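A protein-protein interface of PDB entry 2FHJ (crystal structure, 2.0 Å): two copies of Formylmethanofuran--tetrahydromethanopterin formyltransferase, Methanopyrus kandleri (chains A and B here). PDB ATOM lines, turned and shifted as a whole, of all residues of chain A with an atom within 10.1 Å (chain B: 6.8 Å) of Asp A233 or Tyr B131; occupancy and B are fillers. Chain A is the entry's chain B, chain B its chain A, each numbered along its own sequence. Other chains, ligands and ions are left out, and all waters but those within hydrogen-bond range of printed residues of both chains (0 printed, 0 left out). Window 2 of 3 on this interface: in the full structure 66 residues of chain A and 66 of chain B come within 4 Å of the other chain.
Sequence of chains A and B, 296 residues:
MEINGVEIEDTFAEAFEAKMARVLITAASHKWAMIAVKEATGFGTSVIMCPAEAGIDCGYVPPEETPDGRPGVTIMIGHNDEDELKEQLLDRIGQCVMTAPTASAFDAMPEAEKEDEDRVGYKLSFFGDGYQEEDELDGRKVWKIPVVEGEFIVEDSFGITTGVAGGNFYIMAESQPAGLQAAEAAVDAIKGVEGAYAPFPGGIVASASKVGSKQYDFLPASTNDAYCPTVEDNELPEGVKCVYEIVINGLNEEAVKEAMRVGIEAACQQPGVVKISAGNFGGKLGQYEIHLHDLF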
ATOM      1  N   LYS A 210       5.442  -2.702  -0.554  1.00  0.00           N
ATOM      2  CA  LYS A 210       6.097  -3.124  -1.791  1.00  0.00           C
ATOM      3  C   LYS A 210       7.559  -2.694  -1.713  1.00  0.00           C
ATOM      4  O   LYS A 210       7.900  -1.771  -0.962  1.00  0.00           O
ATOM      5  CB  LYS A 210       5.421  -2.489  -3.013  1.00  0.00           C
ATOM      6  CG  LYS A 210       5.806  -1.030  -3.260  1.00  0.00           C
ATOM      7  CD  LYS A 210       4.732  -0.253  -4.009  1.00  0.00           C
ATOM      8  CE  LYS A 210       5.211   1.141  -4.360  1.00  0.00           C
ATOM      9  NZ  LYS A 210       4.227   2.172  -3.940  1.00  0.00           N
ATOM     10  N   SER A 213       9.897   2.679  -3.738  1.00  0.00           N
ATOM     11  CA  SER A 213       8.846   3.663  -3.954  1.00  0.00           C
ATOM     12  C   SER A 213       8.841   4.115  -5.406  1.00  0.00           C
ATOM     13  O   SER A 213       9.893   4.325  -5.993  1.00  0.00           O
ATOM     14  CB  SER A 213       9.080   4.862  -3.045  1.00  0.00           C
ATOM     15  OG  SER A 213       8.124   5.877  -3.278  1.00  0.00           O
ATOM     16  N   LYS A 214       7.653   4.257  -5.983  1.00  0.00           N
ATOM     17  CA  LYS A 214       7.524   4.783  -7.339  1.00  0.00           C
ATOM     18  C   LYS A 214       7.895   6.255  -7.352  1.00  0.00           C
ATOM     19  O   LYS A 214       8.413   6.752  -8.347  1.00  0.00           O
ATOM     20  CB  LYS A 214       6.092   4.619  -7.878  1.00  0.00           C
ATOM     21  CG  LYS A 214       5.638   3.164  -8.129  1.00  0.00           C
ATOM     22  CD  LYS A 214       4.211   3.101  -8.672  1.00  0.00           C
ATOM     23  N   GLN A 215       7.641   6.941  -6.241  1.00  0.00           N
ATOM     24  CA  GLN A 215       7.764   8.394  -6.179  1.00  0.00           C
ATOM     25  C   GLN A 215       9.056   8.923  -5.542  1.00  0.00           C
ATOM     26  O   GLN A 215       9.508  10.007  -5.895  1.00  0.00           O
ATOM     27  CB  GLN A 215       6.563   8.971  -5.424  1.00  0.00           C
ATOM     28  CG  GLN A 215       6.191  10.369  -5.842  1.00  0.00           C
ATOM     29  CD  GLN A 215       5.682  10.427  -7.269  1.00  0.00           C
ATOM     30  OE1 GLN A 215       5.356   9.402  -7.876  1.00  0.00           O
ATOM     31  NE2 GLN A 215       5.613  11.634  -7.816  1.00  0.00           N
ATOM     32  N   TYR A 216       9.640   8.174  -4.612  1.00  0.00           N
ATOM     33  CA  TYR A 216      10.714   8.699  -3.767  1.00  0.00           C
ATOM     34  C   TYR A 216      12.000   7.875  -3.897  1.00  0.00           C
ATOM     35  O   TYR A 216      11.948   6.674  -4.167  1.00  0.00           O
ATOM     36  CB  TYR A 216      10.238   8.769  -2.307  1.00  0.00           C
ATOM     37  CG  TYR A 216       8.896   9.475  -2.142  1.00  0.00           C
ATOM     38  CD1 TYR A 216       7.758   8.787  -1.721  1.00  0.00           C
ATOM     39  CD2 TYR A 216       8.761  10.829  -2.436  1.00  0.00           C
ATOM     40  CE1 TYR A 216       6.532   9.443  -1.581  1.00  0.00           C
ATOM     41  CE2 TYR A 216       7.541  11.483  -2.306  1.00  0.00           C
ATOM     42  CZ  TYR A 216       6.432  10.785  -1.884  1.00  0.00           C
ATOM     43  OH  TYR A 216       5.233  11.443  -1.750  1.00  0.00           O
ATOM     44  N   LEU A 219      13.326   5.686  -0.010  1.00  0.00           N
ATOM     45  CA  LEU A 219      12.465   4.711   0.664  1.00  0.00           C
ATOM     46  C   LEU A 219      12.807   3.243   0.347  1.00  0.00           C
ATOM     47  O   LEU A 219      12.726   2.821  -0.813  1.00  0.00           O
ATOM     48  CB  LEU A 219      10.982   4.978   0.355  1.00  0.00           C
ATOM     49  CG  LEU A 219      10.254   6.100   1.119  1.00  0.00           C
ATOM     50  CD1 LEU A 219       8.762   5.839   1.092  1.00  0.00           C
ATOM     51  CD2 LEU A 219      10.705   6.262   2.568  1.00  0.00           C
ATOM     52  N   SER A 222       7.451   1.111   0.582  1.00  0.00           N
ATOM     53  CA  SER A 222       6.314   2.029   0.680  1.00  0.00           C
ATOM     54  C   SER A 222       5.047   1.192   0.610  1.00  0.00           C
ATOM     55  O   SER A 222       5.138  -0.031   0.542  1.00  0.00           O
ATOM     56  CB  SER A 222       6.347   3.075  -0.441  1.00  0.00           C
ATOM     57  OG  SER A 222       6.496   2.470  -1.722  1.00  0.00           O
ATOM     58  N   THR A 223       3.880   1.833   0.621  1.00  0.00           N
ATOM     59  CA  THR A 223       2.615   1.089   0.669  1.00  0.00           C
ATOM     60  C   THR A 223       2.302   0.425  -0.660  1.00  0.00           C
ATOM     61  O   THR A 223       2.608   0.976  -1.712  1.00  0.00           O
ATOM     62  CB  THR A 223       1.408   1.972   1.120  1.00  0.00           C
ATOM     63  OG1 THR A 223       0.324   1.127   1.531  1.00  0.00           O
ATOM     64  CG2 THR A 223       0.933   2.897   0.012  1.00  0.00           C
ATOM     65  N   ASN A 224       1.713  -0.771  -0.592  1.00  0.00           N
ATOM     66  CA  ASN A 224       1.291  -1.520  -1.774  1.00  0.00           C
ATOM     67  C   ASN A 224       0.048  -0.868  -2.365  1.00  0.00           C
ATOM     68  O   ASN A 224      -1.081  -1.228  -2.007  1.00  0.00           O
ATOM     69  CB  ASN A 224       1.025  -2.999  -1.446  1.00  0.00           C
ATOM     70  CG  ASN A 224       0.875  -3.879  -2.704  1.00  0.00           C
ATOM     71  OD1 ASN A 224       1.384  -3.548  -3.779  1.00  0.00           O
ATOM     72  ND2 ASN A 224       0.183  -5.010  -2.560  1.00  0.00           N
ATOM     73  N   ASP A 225       0.280   0.100  -3.264  1.00  0.00           N
ATOM     74  CA  ASP A 225      -0.804   0.882  -3.899  1.00  0.00           C
ATOM     75  C   ASP A 225      -1.785   0.003  -4.687  1.00  0.00           C
ATOM     76  O   ASP A 225      -2.960   0.346  -4.832  1.00  0.00           O
ATOM     77  CB  ASP A 225      -0.251   2.033  -4.779  1.00  0.00           C
ATOM     78  CG  ASP A 225       1.036   1.668  -5.527  1.00  0.00           C
ATOM     79  OD1 ASP A 225       2.118   1.677  -4.914  1.00  0.00           O
ATOM     80  OD2 ASP A 225       0.979   1.406  -6.742  1.00  0.00           O
ATOM     81  N   ALA A 226      -1.297  -1.137  -5.165  1.00  0.00           N
ATOM     82  CA  ALA A 226      -2.099  -2.091  -5.922  1.00  0.00           C
ATOM     83  C   ALA A 226      -3.236  -2.707  -5.092  1.00  0.00           C
ATOM     84  O   ALA A 226      -4.288  -3.045  -5.634  1.00  0.00           O
ATOM     85  CB  ALA A 226      -1.195  -3.193  -6.467  1.00  0.00           C
ATOM     86  N   TYR A 227      -3.015  -2.870  -3.788  1.00  0.00           N
ATOM     87  CA  TYR A 227      -4.007  -3.487  -2.894  1.00  0.00           C
ATOM     88  C   TYR A 227      -4.605  -2.511  -1.864  1.00  0.00           C
ATOM     89  O   TYR A 227      -5.239  -2.944  -0.894  1.00  0.00           O
ATOM     90  CB  TYR A 227      -3.369  -4.676  -2.178  1.00  0.00           C
ATOM     91  CG  TYR A 227      -3.237  -5.950  -2.995  1.00  0.00           C
ATOM     92  CD1 TYR A 227      -3.481  -5.978  -4.373  1.00  0.00           C
ATOM     93  CD2 TYR A 227      -2.850  -7.143  -2.378  1.00  0.00           C
ATOM     94  CE1 TYR A 227      -3.352  -7.155  -5.103  1.00  0.00           C
ATOM     95  CE2 TYR A 227      -2.714  -8.325  -3.108  1.00  0.00           C
ATOM     96  CZ  TYR A 227      -2.967  -8.319  -4.468  1.00  0.00           C
ATOM     97  OH  TYR A 227      -2.844  -9.472  -5.192  1.00  0.00           O
ATOM     98  N   CYS A 228      -4.425  -1.207  -2.092  1.00  0.00           N
ATOM     99  CA  CYS A 228      -5.001  -0.173  -1.237  1.00  0.00           C
ATOM    100  C   CYS A 228      -6.380   0.225  -1.714  1.00  0.00           C
ATOM    101  O   CYS A 228      -6.507   0.794  -2.792  1.00  0.00           O
ATOM    102  CB  CYS A 228      -4.123   1.062  -1.231  1.00  0.00           C
ATOM    103  SG  CYS A 228      -2.637   0.801  -0.340  1.00  0.00           S
ATOM    104  N   PRO A 229      -7.420  -0.025  -0.893  1.00  0.00           N
ATOM    105  CA  PRO A 229      -8.784   0.252  -1.338  1.00  0.00           C
ATOM    106  C   PRO A 229      -9.143   1.723  -1.556  1.00  0.00           C
ATOM    107  O   PRO A 229     -10.120   1.987  -2.254  1.00  0.00           O
ATOM    108  CB  PRO A 229      -9.671  -0.354  -0.234  1.00  0.00           C
ATOM    109  CG  PRO A 229      -8.798  -0.774   0.843  1.00  0.00           C
ATOM    110  CD  PRO A 229      -7.371  -0.556   0.478  1.00  0.00           C
ATOM    111  N   THR A 230      -8.402   2.662  -0.970  1.00  0.00           N
ATOM    112  CA  THR A 230      -8.694   4.084  -1.148  1.00  0.00           C
ATOM    113  C   THR A 230      -7.913   4.658  -2.312  1.00  0.00           C
ATOM    114  O   THR A 230      -8.153   5.789  -2.723  1.00  0.00           O
ATOM    115  CB  THR A 230      -8.359   4.911   0.103  1.00  0.00           C
ATOM    116  OG1 THR A 230      -6.980   4.724   0.459  1.00  0.00           O
ATOM    117  CG2 THR A 230      -9.259   4.514   1.264  1.00  0.00           C
ATOM    118  N   VAL A 231      -6.954   3.885  -2.812  1.00  0.00           N
ATOM    119  CA  VAL A 231      -6.229   4.245  -4.021  1.00  0.00           C
ATOM    120  C   VAL A 231      -7.106   3.824  -5.210  1.00  0.00           C
ATOM    121  O   VAL A 231      -7.130   2.655  -5.593  1.00  0.00           O
ATOM    122  CB  VAL A 231      -4.831   3.576  -4.072  1.00  0.00           C
ATOM    123  CG1 VAL A 231      -4.218   3.716  -5.433  1.00  0.00           C
ATOM    124  CG2 VAL A 231      -3.895   4.188  -3.038  1.00  0.00           C
ATOM    125  N   GLU A 232      -7.844   4.786  -5.773  1.00  0.00           N
ATOM    126  CA  GLU A 232      -8.765   4.532  -6.903  1.00  0.00           C
ATOM    127  C   GLU A 232      -7.967   4.351  -8.189  1.00  0.00           C
ATOM    128  O   GLU A 232      -8.256   4.943  -9.228  1.00  0.00           O
ATOM    129  CB  GLU A 232      -9.789   5.670  -7.045  1.00  0.00           C
ATOM    130  CG  GLU A 232     -11.037   5.518  -6.175  1.00  0.00           C
ATOM    131  CD  GLU A 232     -10.730   5.085  -4.756  1.00  0.00           C
ATOM    132  OE1 GLU A 232     -10.454   3.882  -4.552  1.00  0.00           O
ATOM    133  OE2 GLU A 232     -10.776   5.944  -3.850  1.00  0.00           O
ATOM    134  N   ASP A 233      -6.973   3.504  -8.080  1.00  0.00           N
ATOM    135  CA  ASP A 233      -5.929   3.392  -9.050  1.00  0.00           C
ATOM    136  C   ASP A 233      -5.504   1.896  -9.068  1.00  0.00           C
ATOM    137  O   ASP A 233      -4.440   1.553  -9.611  1.00  0.00           O
ATOM    138  CB  ASP A 233      -4.801   4.302  -8.513  1.00  0.00           C
ATOM    139  CG  ASP A 233      -3.998   4.985  -9.586  1.00  0.00           C
ATOM    140  OD1 ASP A 233      -3.337   4.274 -10.373  1.00  0.00           O
ATOM    141  OD2 ASP A 233      -3.973   6.240  -9.596  1.00  0.00           O
ATOM    142  N   ASN A 234      -6.340   0.984  -8.516  1.00  0.00           N
ATOM    143  CA  ASN A 234      -5.861  -0.301  -7.964  1.00  0.00           C
ATOM    144  C   ASN A 234      -6.394  -1.608  -8.532  1.00  0.00           C
ATOM    145  O   ASN A 234      -7.419  -1.643  -9.213  1.00  0.00           O
ATOM    146  CB  ASN A 234      -6.086  -0.317  -6.435  1.00  0.00           C
ATOM    147  CG  ASN A 234      -7.555  -0.409  -6.043  1.00  0.00           C
ATOM    148  OD1 ASN A 234      -8.292  -1.276  -6.514  1.00  0.00           O
ATOM    149  ND2 ASN A 234      -7.980   0.469  -5.148  1.00  0.00           N
ATOM    150  N   GLU A 235      -5.693  -2.690  -8.128  1.00  0.00           N
ATOM    151  CA  GLU A 235      -5.867  -4.032  -8.670  1.00  0.00           C
ATOM    152  C   GLU A 235      -6.756  -4.927  -7.790  1.00  0.00           C
ATOM    153  O   GLU A 235      -6.631  -6.142  -7.813  1.00  0.00           O
ATOM    154  CB  GLU A 235      -4.484  -4.679  -8.860  1.00  0.00           C
ATOM    155  N   LEU A 236      -7.670  -4.337  -7.034  1.00  0.00           N
ATOM    156  CA  LEU A 236      -8.533  -5.117  -6.147  1.00  0.00           C
ATOM    157  C   LEU A 236      -9.859  -5.469  -6.812  1.00  0.00           C
ATOM    158  O   LEU A 236     -10.440  -4.633  -7.516  1.00  0.00           O
ATOM    159  CB  LEU A 236      -8.843  -4.341  -4.861  1.00  0.00           C
ATOM    160  CG  LEU A 236      -7.733  -4.074  -3.845  1.00  0.00           C
ATOM    161  CD1 LEU A 236      -8.252  -3.189  -2.733  1.00  0.00           C
ATOM    162  CD2 LEU A 236      -7.184  -5.376  -3.299  1.00  0.00           C
ATOM    163  N   SER B 125       4.414   9.800   6.311  1.00  0.00           N
ATOM    164  CA  SER B 125       3.450  10.008   5.230  1.00  0.00           C
ATOM    165  C   SER B 125       3.968   9.576   3.852  1.00  0.00           C
ATOM    166  O   SER B 125       3.184   9.183   2.996  1.00  0.00           O
ATOM    167  CB  SER B 125       2.976  11.468   5.196  1.00  0.00           C
ATOM    168  OG  SER B 125       3.997  12.329   4.743  1.00  0.00           O
ATOM    169  N   GLY B 128       2.954   6.452   1.798  1.00  0.00           N
ATOM    170  CA  GLY B 128       1.796   6.504   0.897  1.00  0.00           C
ATOM    171  C   GLY B 128       2.124   6.732  -0.575  1.00  0.00           C
ATOM    172  O   GLY B 128       1.228   6.785  -1.423  1.00  0.00           O
ATOM    173  N   ASP B 129       3.412   6.906  -0.867  1.00  0.00           N
ATOM    174  CA  ASP B 129       3.945   6.967  -2.231  1.00  0.00           C
ATOM    175  C   ASP B 129       3.184   7.894  -3.182  1.00  0.00           C
ATOM    176  O   ASP B 129       2.735   7.485  -4.250  1.00  0.00           O
ATOM    177  CB  ASP B 129       4.032   5.567  -2.817  1.00  0.00           C
ATOM    178  CG  ASP B 129       5.138   5.442  -3.819  1.00  0.00           C
ATOM    179  OD1 ASP B 129       5.941   6.397  -3.916  1.00  0.00           O
ATOM    180  OD2 ASP B 129       5.211   4.395  -4.499  1.00  0.00           O
ATOM    181  N   GLY B 130       3.052   9.149  -2.774  1.00  0.00           N
ATOM    182  CA  GLY B 130       2.339  10.157  -3.546  1.00  0.00           C
ATOM    183  C   GLY B 130       0.858  10.218  -3.253  1.00  0.00           C
ATOM    184  O   GLY B 130       0.246  11.244  -3.509  1.00  0.00           O
ATOM    185  N   TYR B 131       0.290   9.135  -2.710  1.00  0.00           N
ATOM    186  CA  TYR B 131      -1.156   9.034  -2.439  1.00  0.00           C
ATOM    187  C   TYR B 131      -1.597   9.506  -1.039  1.00  0.00           C
ATOM    188  O   TYR B 131      -2.794   9.484  -0.720  1.00  0.00           O
ATOM    189  CB  TYR B 131      -1.610   7.590  -2.622  1.00  0.00           C
ATOM    190  CG  TYR B 131      -1.436   7.040  -4.013  1.00  0.00           C
ATOM    191  CD1 TYR B 131      -0.310   6.295  -4.351  1.00  0.00           C
ATOM    192  CD2 TYR B 131      -2.420   7.232  -4.988  1.00  0.00           C
ATOM    193  CE1 TYR B 131      -0.159   5.767  -5.633  1.00  0.00           C
ATOM    194  CE2 TYR B 131      -2.278   6.708  -6.264  1.00  0.00           C
ATOM    195  CZ  TYR B 131      -1.145   5.979  -6.588  1.00  0.00           C
ATOM    196  OH  TYR B 131      -1.005   5.461  -7.861  1.00  0.00           O
ATOM    197  N   GLN B 132      -0.637   9.913  -0.206  1.00  0.00           N
ATOM    198  CA  GLN B 132      -0.927  10.400   1.145  1.00  0.00           C
ATOM    199  C   GLN B 132      -1.603  11.750   1.122  1.00  0.00           C
ATOM    200  O   GLN B 132      -1.283  12.598   0.291  1.00  0.00           O
ATOM    201  CB  GLN B 132       0.344  10.475   1.996  1.00  0.00           C
ATOM    202  CG  GLN B 132       1.421  11.469   1.538  1.00  0.00           C
ATOM    203  CD  GLN B 132       2.393  10.871   0.548  1.00  0.00           C
ATOM    204  OE1 GLN B 132       2.034  10.002  -0.240  1.00  0.00           O
ATOM    205  NE2 GLN B 132       3.630  11.337   0.581  1.00  0.00           N
ATOM    206  N   GLU B 133      -2.532  11.951   2.049  1.00  0.00           N
ATOM    207  CA  GLU B 133      -3.246  13.216   2.139  1.00  0.00           C
ATOM    208  C   GLU B 133      -3.180  13.772   3.564  1.00  0.00           C
ATOM    209  O   GLU B 133      -3.250  13.032   4.528  1.00  0.00           O
ATOM    210  CB  GLU B 133      -4.709  13.051   1.689  1.00  0.00           C
ATOM    211  CG  GLU B 133      -4.896  12.780   0.177  1.00  0.00           C
ATOM    212  CD  GLU B 133      -4.712  14.024  -0.707  1.00  0.00           C
ATOM    213  OE1 GLU B 133      -5.378  15.049  -0.438  1.00  0.00           O
ATOM    214  OE2 GLU B 133      -3.917  13.971  -1.684  1.00  0.00           O
ATOM    215  N   LYS B 144      -3.499  11.169   6.389  1.00  0.00           N
ATOM    216  CA  LYS B 144      -4.187   9.956   6.000  1.00  0.00           C
ATOM    217  C   LYS B 144      -3.308   9.277   4.972  1.00  0.00           C
ATOM    218  O   LYS B 144      -3.178   9.767   3.860  1.00  0.00           O
ATOM    219  CB  LYS B 144      -5.553  10.287   5.414  1.00  0.00           C
ATOM    220  CG  LYS B 144      -6.380  11.181   6.323  1.00  0.00           C
ATOM    221  CD  LYS B 144      -7.834  11.248   5.917  1.00  0.00           C
ATOM    222  CE  LYS B 144      -8.004  12.030   4.632  1.00  0.00           C
ATOM    223  NZ  LYS B 144      -9.446  12.275   4.329  1.00  0.00           N
ATOM    224  N   ILE B 145      -2.694   8.163   5.372  1.00  0.00           N
ATOM    225  CA  ILE B 145      -1.760   7.401   4.542  1.00  0.00           C
ATOM    226  C   ILE B 145      -2.490   6.163   4.044  1.00  0.00           C
ATOM    227  O   ILE B 145      -3.031   5.406   4.849  1.00  0.00           O
ATOM    228  CB  ILE B 145      -0.528   6.953   5.358  1.00  0.00           C
ATOM    229  CG1 ILE B 145       0.184   8.158   5.975  1.00  0.00           C
ATOM    230  CG2 ILE B 145       0.431   6.142   4.499  1.00  0.00           C
ATOM    231  CD1 ILE B 145       1.316   7.799   6.945  1.00  0.00           C
ATOM    232  N   PRO B 146      -2.551   5.962   2.715  1.00  0.00           N
ATOM    233  CA  PRO B 146      -3.248   4.787   2.200  1.00  0.00           C
ATOM    234  C   PRO B 146      -2.537   3.479   2.516  1.00  0.00           C
ATOM    235  O   PRO B 146      -1.341   3.339   2.256  1.00  0.00           O
ATOM    236  CB  PRO B 146      -3.256   5.019   0.684  1.00  0.00           C
ATOM    237  CG  PRO B 146      -2.951   6.456   0.507  1.00  0.00           C
ATOM    238  CD  PRO B 146      -2.035   6.795   1.612  1.00  0.00           C
ATOM    239  N   GLU B 151      -6.836   3.187   5.646  1.00  0.00           N
ATOM    240  CA  GLU B 151      -5.987   4.357   5.931  1.00  0.00           C
ATOM    241  C   GLU B 151      -5.322   4.294   7.308  1.00  0.00           C
ATOM    242  O   GLU B 151      -5.928   3.835   8.288  1.00  0.00           O
ATOM    243  CB  GLU B 151      -6.810   5.646   5.858  1.00  0.00           C
ATOM    244  CG  GLU B 151      -7.008   6.186   4.446  1.00  0.00           C
ATOM    245  CD  GLU B 151      -7.835   7.468   4.415  1.00  0.00           C
ATOM    246  OE1 GLU B 151      -8.678   7.665   5.329  1.00  0.00           O
ATOM    247  OE2 GLU B 151      -7.638   8.272   3.468  1.00  0.00           O
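The side-chain amide nitrogen of Gln B132 lies within hydrogen-bond range of the side-chain hydroxyl of Tyr A216, at 2.8 Å. The backbone carbonyl oxygen (O) of Pro B146 is in hydrogen-bond range of the side-chain hydroxyl (OG1) of Thr A223 (2.9 Å). The side-chain carboxylate of Asp B129 lies close to the side-chain hydroxyl of Ser A213, 3.5 Å away. The side-chain carboxylate (OD1) of Asp B129 lies within hydrogen-bond range of the backbone NH (N) of Gln A215 (2.9 Å). The side-chain carboxylate of Asp B129 lies within salt-bridge range of the side-chain amino group of Lys A210. The backbone NH (N) of Gly B130 is in hydrogen-bond range of the side-chain hydroxyl (OH) of Tyr A216 (3.3 Å). N of Lys A214 lies within hydrogen-bond range of OD2 of Asp B129, at 2.9 Å.
The backbone NH (N) of Asp B129 lies within hydrogen-bond range of the side-chain amide oxygen (OE1) of Gln B132. OG of Ser A213 lies close to N of Gln A215, 3.2 Å away. SG of Cys A228 sits at hydrogen-bond distance from O of Asn A224. OG1 of Thr A223 lies within hydrogen-bond range of SG of Cys A228 (3.5 Å). N of Gly B130 lies within hydrogen-bond range of OE1 of Gln B132, 2.9 Å away. The backbone NH (N) of Lys A210 is in hydrogen-bond range of the backbone carbonyl oxygen (O) of Ser A222 (2.9 Å).
CA of Asp B129 touches CE1 of Tyr A216, at 3.6 Å. OD2 of Asp B129 touches OG of Ser A222, 3.6 Å away. Gly B128 touches Thr A223. CE1 of Tyr B131 touches CB of Asp A225, at 3.8 Å. SG of Cys A228 touches O of Pro B146, at 3.9 Å. Pro B146 touches Thr A230. CE2 of Tyr B131 touches CG1 of Val A231, at 3.7 Å. Pro B146 touches Val A231 (CB to CG2, 3.9 Å). Tyr B131 touches Asp A233 (OH to CG, 3.5 Å).
Printed residues of chain B within 4 Å of Lys A214: Asp B129. Printed residues of chain B within 4 Å of Asp A225: Tyr B131 (3.8 Å). Printed residues of chain B within 4 Å of Cys A228: Pro B146. Printed residues of chain B within 4 Å of Thr A230: Pro B146. Glu A232 touches none of the printed residues of chain B. Of chain B, only Tyr B131 comes within 4 Å of Asp A233. Of the printed residues of chain A, Asp B129 touches Lys A210 (2.5 Å), Ser A213 (2.3 Å), Lys A214 (2.9 Å), Gln A215 (2.9 Å), Tyr A216 (3.6 Å) and Ser A222 (3.6 Å). Of chain A, only Asp A225 (3.8 Å), Val A231 (3.7 Å) and Asp A233 (3.5 Å) come within 4 Å of Tyr B131. Gln B132 touches one residue of chain A. Ile B145 touches none of the printed residues of chain A. The nearest printed residue of chain B that does not touch Asp A233 is Asp B129 (8.7 Å). The nearest residue of chain A that does not touch Tyr B131 is Tyr A216 (5.5 Å).
Of the 11 printed residues of chain B, 6 touch a printed residue of chain A. Hydrophobic or aromatic side chains of chain B that line the printed part of chain A: Tyr B131 and Pro B146. Hydrophobic or aromatic side chains of chain A that line the printed part of chain B: Tyr A216 and Val A231. Among the printed residues, Asp or Glu carboxylates within 4 Å of a Lys or Arg side-chain nitrogen of the other chain: Lys A210 with Asp B129 (2.5 Å).
No position is printed for both chains.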
